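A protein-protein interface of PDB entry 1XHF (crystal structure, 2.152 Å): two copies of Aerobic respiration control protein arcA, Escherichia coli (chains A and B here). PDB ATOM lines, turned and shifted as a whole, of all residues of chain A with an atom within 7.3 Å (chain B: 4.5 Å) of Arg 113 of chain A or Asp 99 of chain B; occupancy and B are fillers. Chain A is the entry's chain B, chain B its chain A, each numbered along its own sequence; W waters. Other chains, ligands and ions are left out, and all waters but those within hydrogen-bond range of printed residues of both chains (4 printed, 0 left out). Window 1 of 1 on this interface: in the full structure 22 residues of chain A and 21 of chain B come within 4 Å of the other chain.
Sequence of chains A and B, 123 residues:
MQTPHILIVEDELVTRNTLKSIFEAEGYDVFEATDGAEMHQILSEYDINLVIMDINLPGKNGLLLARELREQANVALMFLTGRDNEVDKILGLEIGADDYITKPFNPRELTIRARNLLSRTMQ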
ATOM      1  N   LEU A  50       6.061   1.367  16.708  1.00  0.00           N
ATOM      2  CA  LEU A  50       5.771   2.424  17.651  1.00  0.00           C
ATOM      3  C   LEU A  50       5.727   1.813  19.044  1.00  0.00           C
ATOM      4  O   LEU A  50       5.076   0.788  19.258  1.00  0.00           O
ATOM      5  CB  LEU A  50       4.411   3.100  17.298  1.00  0.00           C
ATOM      6  CG  LEU A  50       3.756   3.989  18.359  1.00  0.00           C
ATOM      7  CD1 LEU A  50       4.652   5.226  18.607  1.00  0.00           C
ATOM      8  CD2 LEU A  50       2.352   4.437  17.930  1.00  0.00           C
ATOM      9  N   MET A  78       6.201   7.127  22.160  1.00  0.00           N
ATOM     10  CA  MET A  78       5.377   8.090  22.881  1.00  0.00           C
ATOM     11  C   MET A  78       5.153   7.640  24.296  1.00  0.00           C
ATOM     12  O   MET A  78       4.785   6.503  24.525  1.00  0.00           O
ATOM     13  CB  MET A  78       4.012   8.308  22.188  1.00  0.00           C
ATOM     14  CG  MET A  78       4.163   8.745  20.740  1.00  0.00           C
ATOM     15  SD  MET A  78       2.376   9.206  19.869  1.00  0.00           S
ATOM     16  CE  MET A  78       1.346   7.914  20.646  1.00  0.00           C
ATOM     17  N   LEU A  93      10.685  13.965  26.763  1.00  0.00           N
ATOM     18  CA  LEU A  93      10.941  14.556  25.446  1.00  0.00           C
ATOM     19  C   LEU A  93      12.450  14.718  25.199  1.00  0.00           C
ATOM     20  O   LEU A  93      12.963  14.339  24.134  1.00  0.00           O
ATOM     21  CB  LEU A  93      10.226  15.919  25.337  1.00  0.00           C
ATOM     22  CG  LEU A  93       8.689  15.797  25.358  1.00  0.00           C
ATOM     23  CD1 LEU A  93       8.008  17.131  25.593  1.00  0.00           C
ATOM     24  CD2 LEU A  93       8.130  15.103  24.074  1.00  0.00           C
ATOM     25  N   ASP A  98       9.058  11.051  20.883  1.00  0.00           N
ATOM     26  CA  ASP A  98       8.399  11.895  19.898  1.00  0.00           C
ATOM     27  C   ASP A  98       7.180  12.565  20.492  1.00  0.00           C
ATOM     28  O   ASP A  98       6.740  13.592  20.008  1.00  0.00           O
ATOM     29  CB  ASP A  98       8.005  11.062  18.676  1.00  0.00           C
ATOM     30  CG  ASP A  98       9.204  10.490  18.001  1.00  0.00           C
ATOM     31  OD1 ASP A  98       9.506   9.307  18.217  1.00  0.00           O
ATOM     32  OD2 ASP A  98       9.945  11.180  17.274  1.00  0.00           O
ATOM     33  N   ASP A  99       6.619  11.992  21.542  1.00  0.00           N
ATOM     34  CA  ASP A  99       5.495  12.673  22.155  1.00  0.00           C
ATOM     35  C   ASP A  99       5.352  12.270  23.583  1.00  0.00           C
ATOM     36  O   ASP A  99       5.978  11.303  24.016  1.00  0.00           O
ATOM     37  CB  ASP A  99       4.211  12.332  21.412  1.00  0.00           C
ATOM     38  CG  ASP A  99       3.267  13.518  21.316  1.00  0.00           C
ATOM     39  OD1 ASP A  99       2.634  13.620  20.246  1.00  0.00           O
ATOM     40  OD2 ASP A  99       3.109  14.378  22.244  1.00  0.00           O
ATOM     41  N   TYR A 100       4.519  12.992  24.322  1.00  0.00           N
ATOM     42  CA  TYR A 100       4.333  12.720  25.749  1.00  0.00           C
ATOM     43  C   TYR A 100       2.875  13.037  26.061  1.00  0.00           C
ATOM     44  O   TYR A 100       2.436  14.184  25.978  1.00  0.00           O
ATOM     45  CB  TYR A 100       5.281  13.607  26.593  1.00  0.00           C
ATOM     46  CG  TYR A 100       5.303  13.285  28.085  1.00  0.00           C
ATOM     47  CD1 TYR A 100       6.353  12.540  28.633  1.00  0.00           C
ATOM     48  CD2 TYR A 100       4.271  13.714  28.950  1.00  0.00           C
ATOM     49  CE1 TYR A 100       6.391  12.197  29.969  1.00  0.00           C
ATOM     50  CE2 TYR A 100       4.301  13.381  30.321  1.00  0.00           C
ATOM     51  CZ  TYR A 100       5.394  12.627  30.817  1.00  0.00           C
ATOM     52  OH  TYR A 100       5.487  12.266  32.153  1.00  0.00           O
ATOM     53  N   ILE A 101       2.120  12.022  26.412  1.00  0.00           N
ATOM     54  CA  ILE A 101       0.694  12.177  26.622  1.00  0.00           C
ATOM     55  C   ILE A 101       0.335  11.729  28.026  1.00  0.00           C
ATOM     56  O   ILE A 101       0.822  10.704  28.489  1.00  0.00           O
ATOM     57  CB  ILE A 101      -0.087  11.340  25.544  1.00  0.00           C
ATOM     58  CG1 ILE A 101       0.324  11.815  24.143  1.00  0.00           C
ATOM     59  CG2 ILE A 101      -1.622  11.347  25.826  1.00  0.00           C
ATOM     60  CD1 ILE A 101       0.054  10.805  23.052  1.00  0.00           C
ATOM     61  N   PRO A 107      -8.833   9.376  23.563  1.00  0.00           N
ATOM     62  CA  PRO A 107      -8.373   8.325  22.650  1.00  0.00           C
ATOM     63  C   PRO A 107      -8.205   8.818  21.222  1.00  0.00           C
ATOM     64  O   PRO A 107      -7.325   8.287  20.554  1.00  0.00           O
ATOM     65  CB  PRO A 107      -9.477   7.252  22.743  1.00  0.00           C
ATOM     66  CG  PRO A 107     -10.225   7.573  24.052  1.00  0.00           C
ATOM     67  CD  PRO A 107     -10.136   9.069  24.196  1.00  0.00           C
ATOM     68  N   ARG A 108      -9.017   9.770  20.737  1.00  0.00           N
ATOM     69  CA  ARG A 108      -8.792  10.303  19.374  1.00  0.00           C
ATOM     70  C   ARG A 108      -7.468  10.998  19.276  1.00  0.00           C
ATOM     71  O   ARG A 108      -6.795  10.936  18.256  1.00  0.00           O
ATOM     72  CB  ARG A 108      -9.885  11.312  18.928  1.00  0.00           C
ATOM     73  CG  ARG A 108     -11.254  10.760  18.887  1.00  0.00           C
ATOM     74  CD  ARG A 108     -11.408   9.451  18.111  1.00  0.00           C
ATOM     75  NE  ARG A 108     -12.780   8.973  18.304  1.00  0.00           N
ATOM     76  CZ  ARG A 108     -13.189   7.707  18.294  1.00  0.00           C
ATOM     77  NH1 ARG A 108     -14.488   7.457  18.464  1.00  0.00           N
ATOM     78  NH2 ARG A 108     -12.324   6.703  18.096  1.00  0.00           N
ATOM     79  N   GLU A 109      -7.101  11.699  20.338  1.00  0.00           N
ATOM     80  CA  GLU A 109      -5.855  12.430  20.304  1.00  0.00           C
ATOM     81  C   GLU A 109      -4.691  11.455  20.238  1.00  0.00           C
ATOM     82  O   GLU A 109      -3.765  11.645  19.471  1.00  0.00           O
ATOM     83  CB  GLU A 109      -5.711  13.378  21.520  1.00  0.00           C
ATOM     84  CG  GLU A 109      -4.392  14.146  21.417  1.00  0.00           C
ATOM     85  CD  GLU A 109      -4.058  15.050  22.603  1.00  0.00           C
ATOM     86  OE1 GLU A 109      -2.964  15.637  22.581  1.00  0.00           O
ATOM     87  OE2 GLU A 109      -4.861  15.164  23.547  1.00  0.00           O
ATOM     88  N   LEU A 110      -4.745  10.415  21.066  1.00  0.00           N
ATOM     89  CA  LEU A 110      -3.748   9.366  21.045  1.00  0.00           C
ATOM     90  C   LEU A 110      -3.633   8.744  19.650  1.00  0.00           C
ATOM     91  O   LEU A 110      -2.544   8.638  19.108  1.00  0.00           O
ATOM     92  CB  LEU A 110      -4.107   8.295  22.091  1.00  0.00           C
ATOM     93  CG  LEU A 110      -3.199   7.065  22.169  1.00  0.00           C
ATOM     94  CD1 LEU A 110      -1.733   7.461  22.532  1.00  0.00           C
ATOM     95  CD2 LEU A 110      -3.763   6.037  23.159  1.00  0.00           C
ATOM     96  N   THR A 111      -4.751   8.349  19.028  1.00  0.00           N
ATOM     97  CA  THR A 111      -4.594   7.640  17.761  1.00  0.00           C
ATOM     98  C   THR A 111      -4.206   8.524  16.610  1.00  0.00           C
ATOM     99  O   THR A 111      -3.558   8.062  15.695  1.00  0.00           O
ATOM    100  CB  THR A 111      -5.872   6.864  17.356  1.00  0.00           C
ATOM    101  OG1 THR A 111      -6.999   7.743  17.429  1.00  0.00           O
ATOM    102  CG2 THR A 111      -6.164   5.727  18.352  1.00  0.00           C
ATOM    103  N   ILE A 112      -4.592   9.797  16.637  1.00  0.00           N
ATOM    104  CA  ILE A 112      -4.191  10.683  15.539  1.00  0.00           C
ATOM    105  C   ILE A 112      -2.701  11.047  15.643  1.00  0.00           C
ATOM    106  O   ILE A 112      -1.973  11.029  14.642  1.00  0.00           O
ATOM    107  CB  ILE A 112      -5.124  11.965  15.514  1.00  0.00           C
ATOM    108  CG1 ILE A 112      -6.548  11.571  15.078  1.00  0.00           C
ATOM    109  CG2 ILE A 112      -4.589  12.975  14.506  1.00  0.00           C
ATOM    110  CD1 ILE A 112      -7.660  12.622  15.565  1.00  0.00           C
ATOM    111  N   ARG A 113      -2.214  11.300  16.864  1.00  0.00           N
ATOM    112  CA  ARG A 113      -0.774  11.502  17.066  1.00  0.00           C
ATOM    113  C   ARG A 113       0.042  10.258  16.649  1.00  0.00           C
ATOM    114  O   ARG A 113       1.058  10.373  15.974  1.00  0.00           O
ATOM    115  CB  ARG A 113      -0.483  11.862  18.537  1.00  0.00           C
ATOM    116  CG  ARG A 113      -0.966  13.264  18.998  1.00  0.00           C
ATOM    117  CD  ARG A 113      -0.649  13.576  20.484  1.00  0.00           C
ATOM    118  NE  ARG A 113      -1.025  14.959  20.860  1.00  0.00           N
ATOM    119  CZ  ARG A 113      -0.262  16.025  20.671  1.00  0.00           C
ATOM    120  NH1 ARG A 113       0.943  15.879  20.128  1.00  0.00           N
ATOM    121  NH2 ARG A 113      -0.712  17.236  21.011  1.00  0.00           N
ATOM    122  N   ALA A 114      -0.436   9.065  16.993  1.00  0.00           N
ATOM    123  CA  ALA A 114       0.230   7.813  16.590  1.00  0.00           C
ATOM    124  C   ALA A 114       0.267   7.722  15.075  1.00  0.00           C
ATOM    125  O   ALA A 114       1.323   7.441  14.473  1.00  0.00           O
ATOM    126  CB  ALA A 114      -0.504   6.636  17.195  1.00  0.00           C
ATOM    127  N   ARG A 115      -0.884   7.982  14.444  1.00  0.00           N
ATOM    128  CA  ARG A 115      -0.973   7.916  12.993  1.00  0.00           C
ATOM    129  C   ARG A 115      -0.038   8.918  12.296  1.00  0.00           C
ATOM    130  O   ARG A 115       0.692   8.551  11.368  1.00  0.00           O
ATOM    131  CB  ARG A 115      -2.440   8.102  12.537  1.00  0.00           C
ATOM    132  CG  ARG A 115      -2.642   8.038  10.996  1.00  0.00           C
ATOM    133  CD  ARG A 115      -3.823   8.935  10.484  1.00  0.00           C
ATOM    134  NE  ARG A 115      -3.493  10.381  10.471  1.00  0.00           N
ATOM    135  CZ  ARG A 115      -4.394  11.388  10.642  1.00  0.00           C
ATOM    136  NH1 ARG A 115      -5.675  11.078  10.847  1.00  0.00           N
ATOM    137  NH2 ARG A 115      -4.008  12.699  10.563  1.00  0.00           N
ATOM    138  N   ASN A 116      -0.040  10.185  12.725  1.00  0.00           N
ATOM    139  CA  ASN A 116       0.890  11.139  12.094  1.00  0.00           C
ATOM    140  C   ASN A 116       2.338  10.729  12.336  1.00  0.00           C
ATOM    141  O   ASN A 116       3.167  10.852  11.469  1.00  0.00           O
ATOM    142  CB  ASN A 116       0.666  12.597  12.563  1.00  0.00           C
ATOM    143  CG  ASN A 116      -0.759  13.129  12.214  1.00  0.00           C
ATOM    144  OD1 ASN A 116      -1.419  12.636  11.296  1.00  0.00           O
ATOM    145  ND2 ASN A 116      -1.222  14.108  12.964  1.00  0.00           N
ATOM    146  N   LEU A 117       2.639  10.259  13.534  1.00  0.00           N
ATOM    147  CA  LEU A 117       4.013   9.828  13.834  1.00  0.00           C
ATOM    148  C   LEU A 117       4.417   8.621  12.942  1.00  0.00           C
ATOM    149  O   LEU A 117       5.492   8.589  12.330  1.00  0.00           O
ATOM    150  CB  LEU A 117       4.124   9.493  15.328  1.00  0.00           C
ATOM    151  CG  LEU A 117       5.510   9.118  15.880  1.00  0.00           C
ATOM    152  CD1 LEU A 117       6.618  10.109  15.433  1.00  0.00           C
ATOM    153  CD2 LEU A 117       5.459   8.964  17.411  1.00  0.00           C
ATOM    154  N   LEU A 118       3.530   7.649  12.823  1.00  0.00           N
ATOM    155  CA  LEU A 118       3.819   6.497  11.968  1.00  0.00           C
ATOM    156  C   LEU A 118       3.991   6.876  10.503  1.00  0.00           C
ATOM    157  O   LEU A 118       4.829   6.278   9.818  1.00  0.00           O
ATOM    158  CB  LEU A 118       2.718   5.449  12.097  1.00  0.00           C
ATOM    159  CG  LEU A 118       2.644   4.689  13.427  1.00  0.00           C
ATOM    160  CD1 LEU A 118       1.270   4.027  13.599  1.00  0.00           C
ATOM    161  CD2 LEU A 118       3.714   3.641  13.489  1.00  0.00           C
ATOM    162  N   SER A 119       3.183   7.829  10.020  1.00  0.00           N
ATOM    163  CA  SER A 119       3.272   8.319   8.632  1.00  0.00           C
ATOM    164  C   SER A 119       4.636   8.902   8.421  1.00  0.00           C
ATOM    165  O   SER A 119       5.196   8.803   7.336  1.00  0.00           O
ATOM    166  CB  SER A 119       2.216   9.417   8.308  1.00  0.00           C
ATOM    167  OG  SER A 119       0.905   8.849   8.262  1.00  0.00           O
ATOM    168  N   LEU B  77       5.317  20.490  10.846  1.00  0.00           N
ATOM    169  CA  LEU B  77       4.374  21.516  11.228  1.00  0.00           C
ATOM    170  C   LEU B  77       3.888  21.380  12.663  1.00  0.00           C
ATOM    171  O   LEU B  77       3.432  20.325  13.068  1.00  0.00           O
ATOM    172  CB  LEU B  77       3.179  21.508  10.255  1.00  0.00           C
ATOM    173  CG  LEU B  77       1.939  22.315  10.658  1.00  0.00           C
ATOM    174  CD1 LEU B  77       2.173  23.757  10.396  1.00  0.00           C
ATOM    175  CD2 LEU B  77       0.714  21.824   9.847  1.00  0.00           C
ATOM    176  N   MET B  78       3.935  22.470  13.413  1.00  0.00           N
ATOM    177  CA  MET B  78       3.377  22.448  14.742  1.00  0.00           C
ATOM    178  C   MET B  78       2.504  23.650  14.913  1.00  0.00           C
ATOM    179  O   MET B  78       2.903  24.750  14.557  1.00  0.00           O
ATOM    180  CB  MET B  78       4.494  22.455  15.825  1.00  0.00           C
ATOM    181  CG  MET B  78       5.463  21.278  15.644  1.00  0.00           C
ATOM    182  SD  MET B  78       6.799  21.113  17.153  1.00  0.00           S
ATOM    183  CE  MET B  78       7.417  22.804  17.120  1.00  0.00           C
ATOM    184  N   PHE B  79       1.313  23.432  15.444  1.00  0.00           N
ATOM    185  CA  PHE B  79       0.479  24.532  15.867  1.00  0.00           C
ATOM    186  C   PHE B  79       0.968  25.011  17.194  1.00  0.00           C
ATOM    187  O   PHE B  79       1.381  24.203  18.074  1.00  0.00           O
ATOM    188  CB  PHE B  79      -0.961  24.075  16.042  1.00  0.00           C
ATOM    189  CG  PHE B  79      -1.691  23.950  14.751  1.00  0.00           C
ATOM    190  CD1 PHE B  79      -1.915  22.710  14.193  1.00  0.00           C
ATOM    191  CD2 PHE B  79      -2.102  25.074  14.067  1.00  0.00           C
ATOM    192  CE1 PHE B  79      -2.601  22.582  12.990  1.00  0.00           C
ATOM    193  CE2 PHE B  79      -2.789  24.948  12.854  1.00  0.00           C
ATOM    194  CZ  PHE B  79      -3.037  23.705  12.328  1.00  0.00           C
ATOM    195  N   LEU B  93      -4.387  18.315  14.621  1.00  0.00           N
ATOM    196  CA  LEU B  93      -3.693  17.033  14.455  1.00  0.00           C
ATOM    197  C   LEU B  93      -4.273  16.252  13.274  1.00  0.00           C
ATOM    198  O   LEU B  93      -3.516  15.754  12.417  1.00  0.00           O
ATOM    199  CB  LEU B  93      -3.752  16.223  15.748  1.00  0.00           C
ATOM    200  CG  LEU B  93      -3.105  16.899  16.962  1.00  0.00           C
ATOM    201  CD1 LEU B  93      -3.562  16.190  18.260  1.00  0.00           C
ATOM    202  CD2 LEU B  93      -1.575  16.942  16.861  1.00  0.00           C
ATOM    203  N   ALA B  97      -0.880  18.246  11.379  1.00  0.00           N
ATOM    204  CA  ALA B  97       0.176  18.877  12.165  1.00  0.00           C
ATOM    205  C   ALA B  97       0.871  17.776  12.973  1.00  0.00           C
ATOM    206  O   ALA B  97       0.207  16.903  13.551  1.00  0.00           O
ATOM    207  CB  ALA B  97      -0.351  19.922  13.085  1.00  0.00           C
ATOM    208  N   ASP B  98       2.201  17.816  12.979  1.00  0.00           N
ATOM    209  CA  ASP B  98       2.986  16.914  13.813  1.00  0.00           C
ATOM    210  C   ASP B  98       2.839  17.201  15.302  1.00  0.00           C
ATOM    211  O   ASP B  98       3.071  16.325  16.136  1.00  0.00           O
ATOM    212  CB  ASP B  98       4.464  16.995  13.448  1.00  0.00           C
ATOM    213  CG  ASP B  98       4.713  16.562  12.069  1.00  0.00           C
ATOM    214  OD1 ASP B  98       4.834  17.433  11.173  1.00  0.00           O
ATOM    215  OD2 ASP B  98       4.779  15.345  11.775  1.00  0.00           O
ATOM    216  N   ASP B  99       2.489  18.419  15.659  1.00  0.00           N
ATOM    217  CA  ASP B  99       2.203  18.680  17.056  1.00  0.00           C
ATOM    218  C   ASP B  99       1.247  19.826  17.211  1.00  0.00           C
ATOM    219  O   ASP B  99       1.009  20.569  16.277  1.00  0.00           O
ATOM    220  CB  ASP B  99       3.484  19.043  17.800  1.00  0.00           C
ATOM    221  CG  ASP B  99       3.549  18.411  19.177  1.00  0.00           C
ATOM    222  OD1 ASP B  99       2.531  18.420  19.967  1.00  0.00           O
ATOM    223  OD2 ASP B  99       4.614  17.885  19.545  1.00  0.00           O
ATOM    224  N   TYR B 100       0.754  19.999  18.419  1.00  0.00           N
ATOM    225  CA  TYR B 100      -0.166  21.068  18.717  1.00  0.00           C
ATOM    226  C   TYR B 100       0.128  21.545  20.122  1.00  0.00           C
ATOM    227  O   TYR B 100      -0.049  20.787  21.065  1.00  0.00           O
ATOM    228  CB  TYR B 100      -1.604  20.524  18.678  1.00  0.00           C
ATOM    229  CG  TYR B 100      -2.687  21.578  18.721  1.00  0.00           C
ATOM    230  CD1 TYR B 100      -3.366  21.958  17.557  1.00  0.00           C
ATOM    231  CD2 TYR B 100      -3.063  22.168  19.918  1.00  0.00           C
ATOM    232  CE1 TYR B 100      -4.352  22.899  17.594  1.00  0.00           C
ATOM    233  CE2 TYR B 100      -4.075  23.120  19.966  1.00  0.00           C
ATOM    234  CZ  TYR B 100      -4.712  23.477  18.797  1.00  0.00           C
ATOM    235  OH  TYR B 100      -5.727  24.415  18.846  1.00  0.00           O
ATOM    236  N   ILE B 101       0.556  22.794  20.260  1.00  0.00           N
ATOM    237  CA  ILE B 101       1.003  23.300  21.539  1.00  0.00           C
ATOM    238  C   ILE B 101       0.208  24.533  21.896  1.00  0.00           C
ATOM    239  O   ILE B 101      -0.040  25.388  21.043  1.00  0.00           O
ATOM    240  CB  ILE B 101       2.513  23.609  21.493  1.00  0.00           C
ATOM    241  CG1 ILE B 101       3.288  22.316  21.218  1.00  0.00           C
ATOM    242  CG2 ILE B 101       2.945  24.278  22.801  1.00  0.00           C
ATOM    243  CD1 ILE B 101       4.698  22.524  20.560  1.00  0.00           C
ATOM    244  N   ARG B 113      10.561  19.700  21.437  1.00  0.00           N
ATOM    245  CA  ARG B 113       9.682  19.023  20.476  1.00  0.00           C
ATOM    246  C   ARG B 113      10.143  19.370  19.052  1.00  0.00           C
ATOM    247  O   ARG B 113      10.177  18.513  18.175  1.00  0.00           O
ATOM    248  CB  ARG B 113       8.215  19.429  20.692  1.00  0.00           C
ATOM    249  CG  ARG B 113       7.535  18.695  21.838  1.00  0.00           C
ATOM    250  CD  ARG B 113       6.139  19.279  22.177  1.00  0.00           C
ATOM    251  NE  ARG B 113       5.467  18.626  23.303  1.00  0.00           N
ATOM    252  CZ  ARG B 113       4.787  17.486  23.247  1.00  0.00           C
ATOM    253  NH1 ARG B 113       4.682  16.784  22.108  1.00  0.00           N
ATOM    254  NH2 ARG B 113       4.192  17.049  24.350  1.00  0.00           N
HETATM  255  O   HOH W   1       1.337  15.898  23.651  1.00  0.00           O
HETATM  256  O   HOH W   2       1.712  18.581  22.685  1.00  0.00           O
HETATM  257  O   HOH W   3       0.526  14.563  15.585  1.00  0.00           O
HETATM  258  O   HOH W   4       2.596  13.000  15.399  1.00  0.00           O
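The side-chain carboxylate (OE1) of Glu 109 of chain A lies within salt-bridge range of the guanidinium group (NE) of Arg 113 of chain A (2.7 Å).
NH1 of Arg 113 of chain A is in salt-bridge range of OD1 of Asp 99 of chain A (2.8 Å).
The guanidinium group (NH1) of Arg 113 of chain B lies within salt-bridge range of the side-chain carboxylate (OD2) of Asp 99 of chain B (2.8 Å).
N of Asp 99 of chain B sits at hydrogen-bond distance from O of Leu 77 of chain B.
The side-chain amide oxygen (OD1) of Asn 116 of chain A is in hydrogen-bond range of the guanidinium group (NH2) of Arg 115 of chain A (2.7 Å).
The side-chain hydroxyl of Ser 119 of chain A lies within hydrogen-bond range of the backbone carbonyl oxygen of Arg 115 of chain A.
Among the printed residues, merely in contact across the chains: Ile 112 of chain A with Leu 93 of chain B (3.5 Å), Arg 115 of chain A with Leu 93 of chain B (3.6 Å), Arg 113 of chain A with Tyr 100 of chain B (3.6 Å), Leu 93 of chain A with Arg 113 of chain B (3.7 Å), Tyr 100 of chain A with Arg 113 of chain B (3.7 Å), Arg 113 of chain A with Leu 93 of chain B (3.8 Å) and Glu 109 of chain A with Leu 93 of chain B (3.9 Å).
The backbone carbonyl oxygen (O) of Leu 93 of chain B lies within hydrogen-bond range of the side-chain amide nitrogen (ND2) of Asn 116 of chain A (2.9 Å).
The backbone carbonyl oxygen (O) of Ala 97 of chain B is in hydrogen-bond range of the side-chain amide nitrogen (ND2) of Asn 116 of chain A (3.2 Å).
The guanidinium group of Arg 113 of chain B lies within salt-bridge range of the side-chain carboxylate of Asp 99 of chain A (2.9 Å).
OD1 of Asp 99 of chain B lies within salt-bridge range of NH1 of Arg 113 of chain A, at 3.0 Å.
Arg 113 of chain A touches just these residues of chain B: Leu 93 (3.8 Å), Asp 99 (3.0 Å) and Tyr 100 (3.6 Å).
Of chain A, only Arg 113 comes within 4 Å of Asp 99 of chain B.
Of the printed residues of chain A, Tyr 100 of chain B touches Arg 113.
Of the printed residues of chain A, Arg 113 of chain B touches Leu 93 (3.7 Å), Asp 99 (2.9 Å) and Tyr 100 (3.7 Å).
Leu 77 of chain B touches none of the printed residues of chain A.
The nearest residue of chain A that does not touch Asp 99 of chain B is Asp 99 of chain A (4.7 Å).
Leu 93 of chain A touches Arg 113 of chain B, and with the chains exchanged Arg 113 of chain A touches Leu 93 of chain B.
Asp 99 of chain A touches Arg 113 of chain B, and with the chains exchanged Arg 113 of chain A touches Asp 99 of chain B.
Tyr 100 of chain A touches Arg 113 of chain B, and with the chains exchanged Arg 113 of chain A touches Tyr 100 of chain B.
Of the 11 pairs that touch across the chains among the printed residues, 6 have their exchanged pair printed and touching as well.
Water W1 lies within hydrogen-bond range of the side-chain carboxylate (OD2) of Asp 99 of chain A (2.7 Å), the backbone carbonyl oxygen (O) of Tyr 100 of chain A (3.1 Å) and the guanidinium group (NH2) of Arg 113 of chain B (3.2 Å).
Water W2 lies within hydrogen-bond range of OD1 of Asp 99 of chain B, NH2 of Arg 113 of chain A, O of Tyr 100 of chain B and NH2 of Arg 113 of chain B.
Water W4 lies within hydrogen-bond range of O of Arg 113 of chain A (3.1 Å), N of Leu 117 of chain A (3.3 Å) and O of Asp 98 of chain B (3.4 Å).
Water W3 lies within hydrogen-bond range of O of Ala 97 of chain B (3.1 Å), O of Asp 98 of chain B (3.1 Å) and ND2 of Asn 116 of chain A (3.2 Å).
Of the 20 printed residues of chain A, 8 touch a printed residue of chain B.
Printed residues of chain A that touch a printed residue of chain B: Leu 93, Asp 99, Tyr 100, Glu 109, Ile 112, Arg 113, Arg 115 and Asn 116.
Hydrophobic or aromatic side chains of chain A within 4 Å of the printed part of chain B: Leu 93 and Ile 112.
Along chain A the printed residues that touch a printed residue of chain B span positions 93 to 116.
Hydrophobic or aromatic side chains of chain B within 4 Å of the printed part of chain A: Leu 93.
Among the printed residues, 11 pairs touch across the chains.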
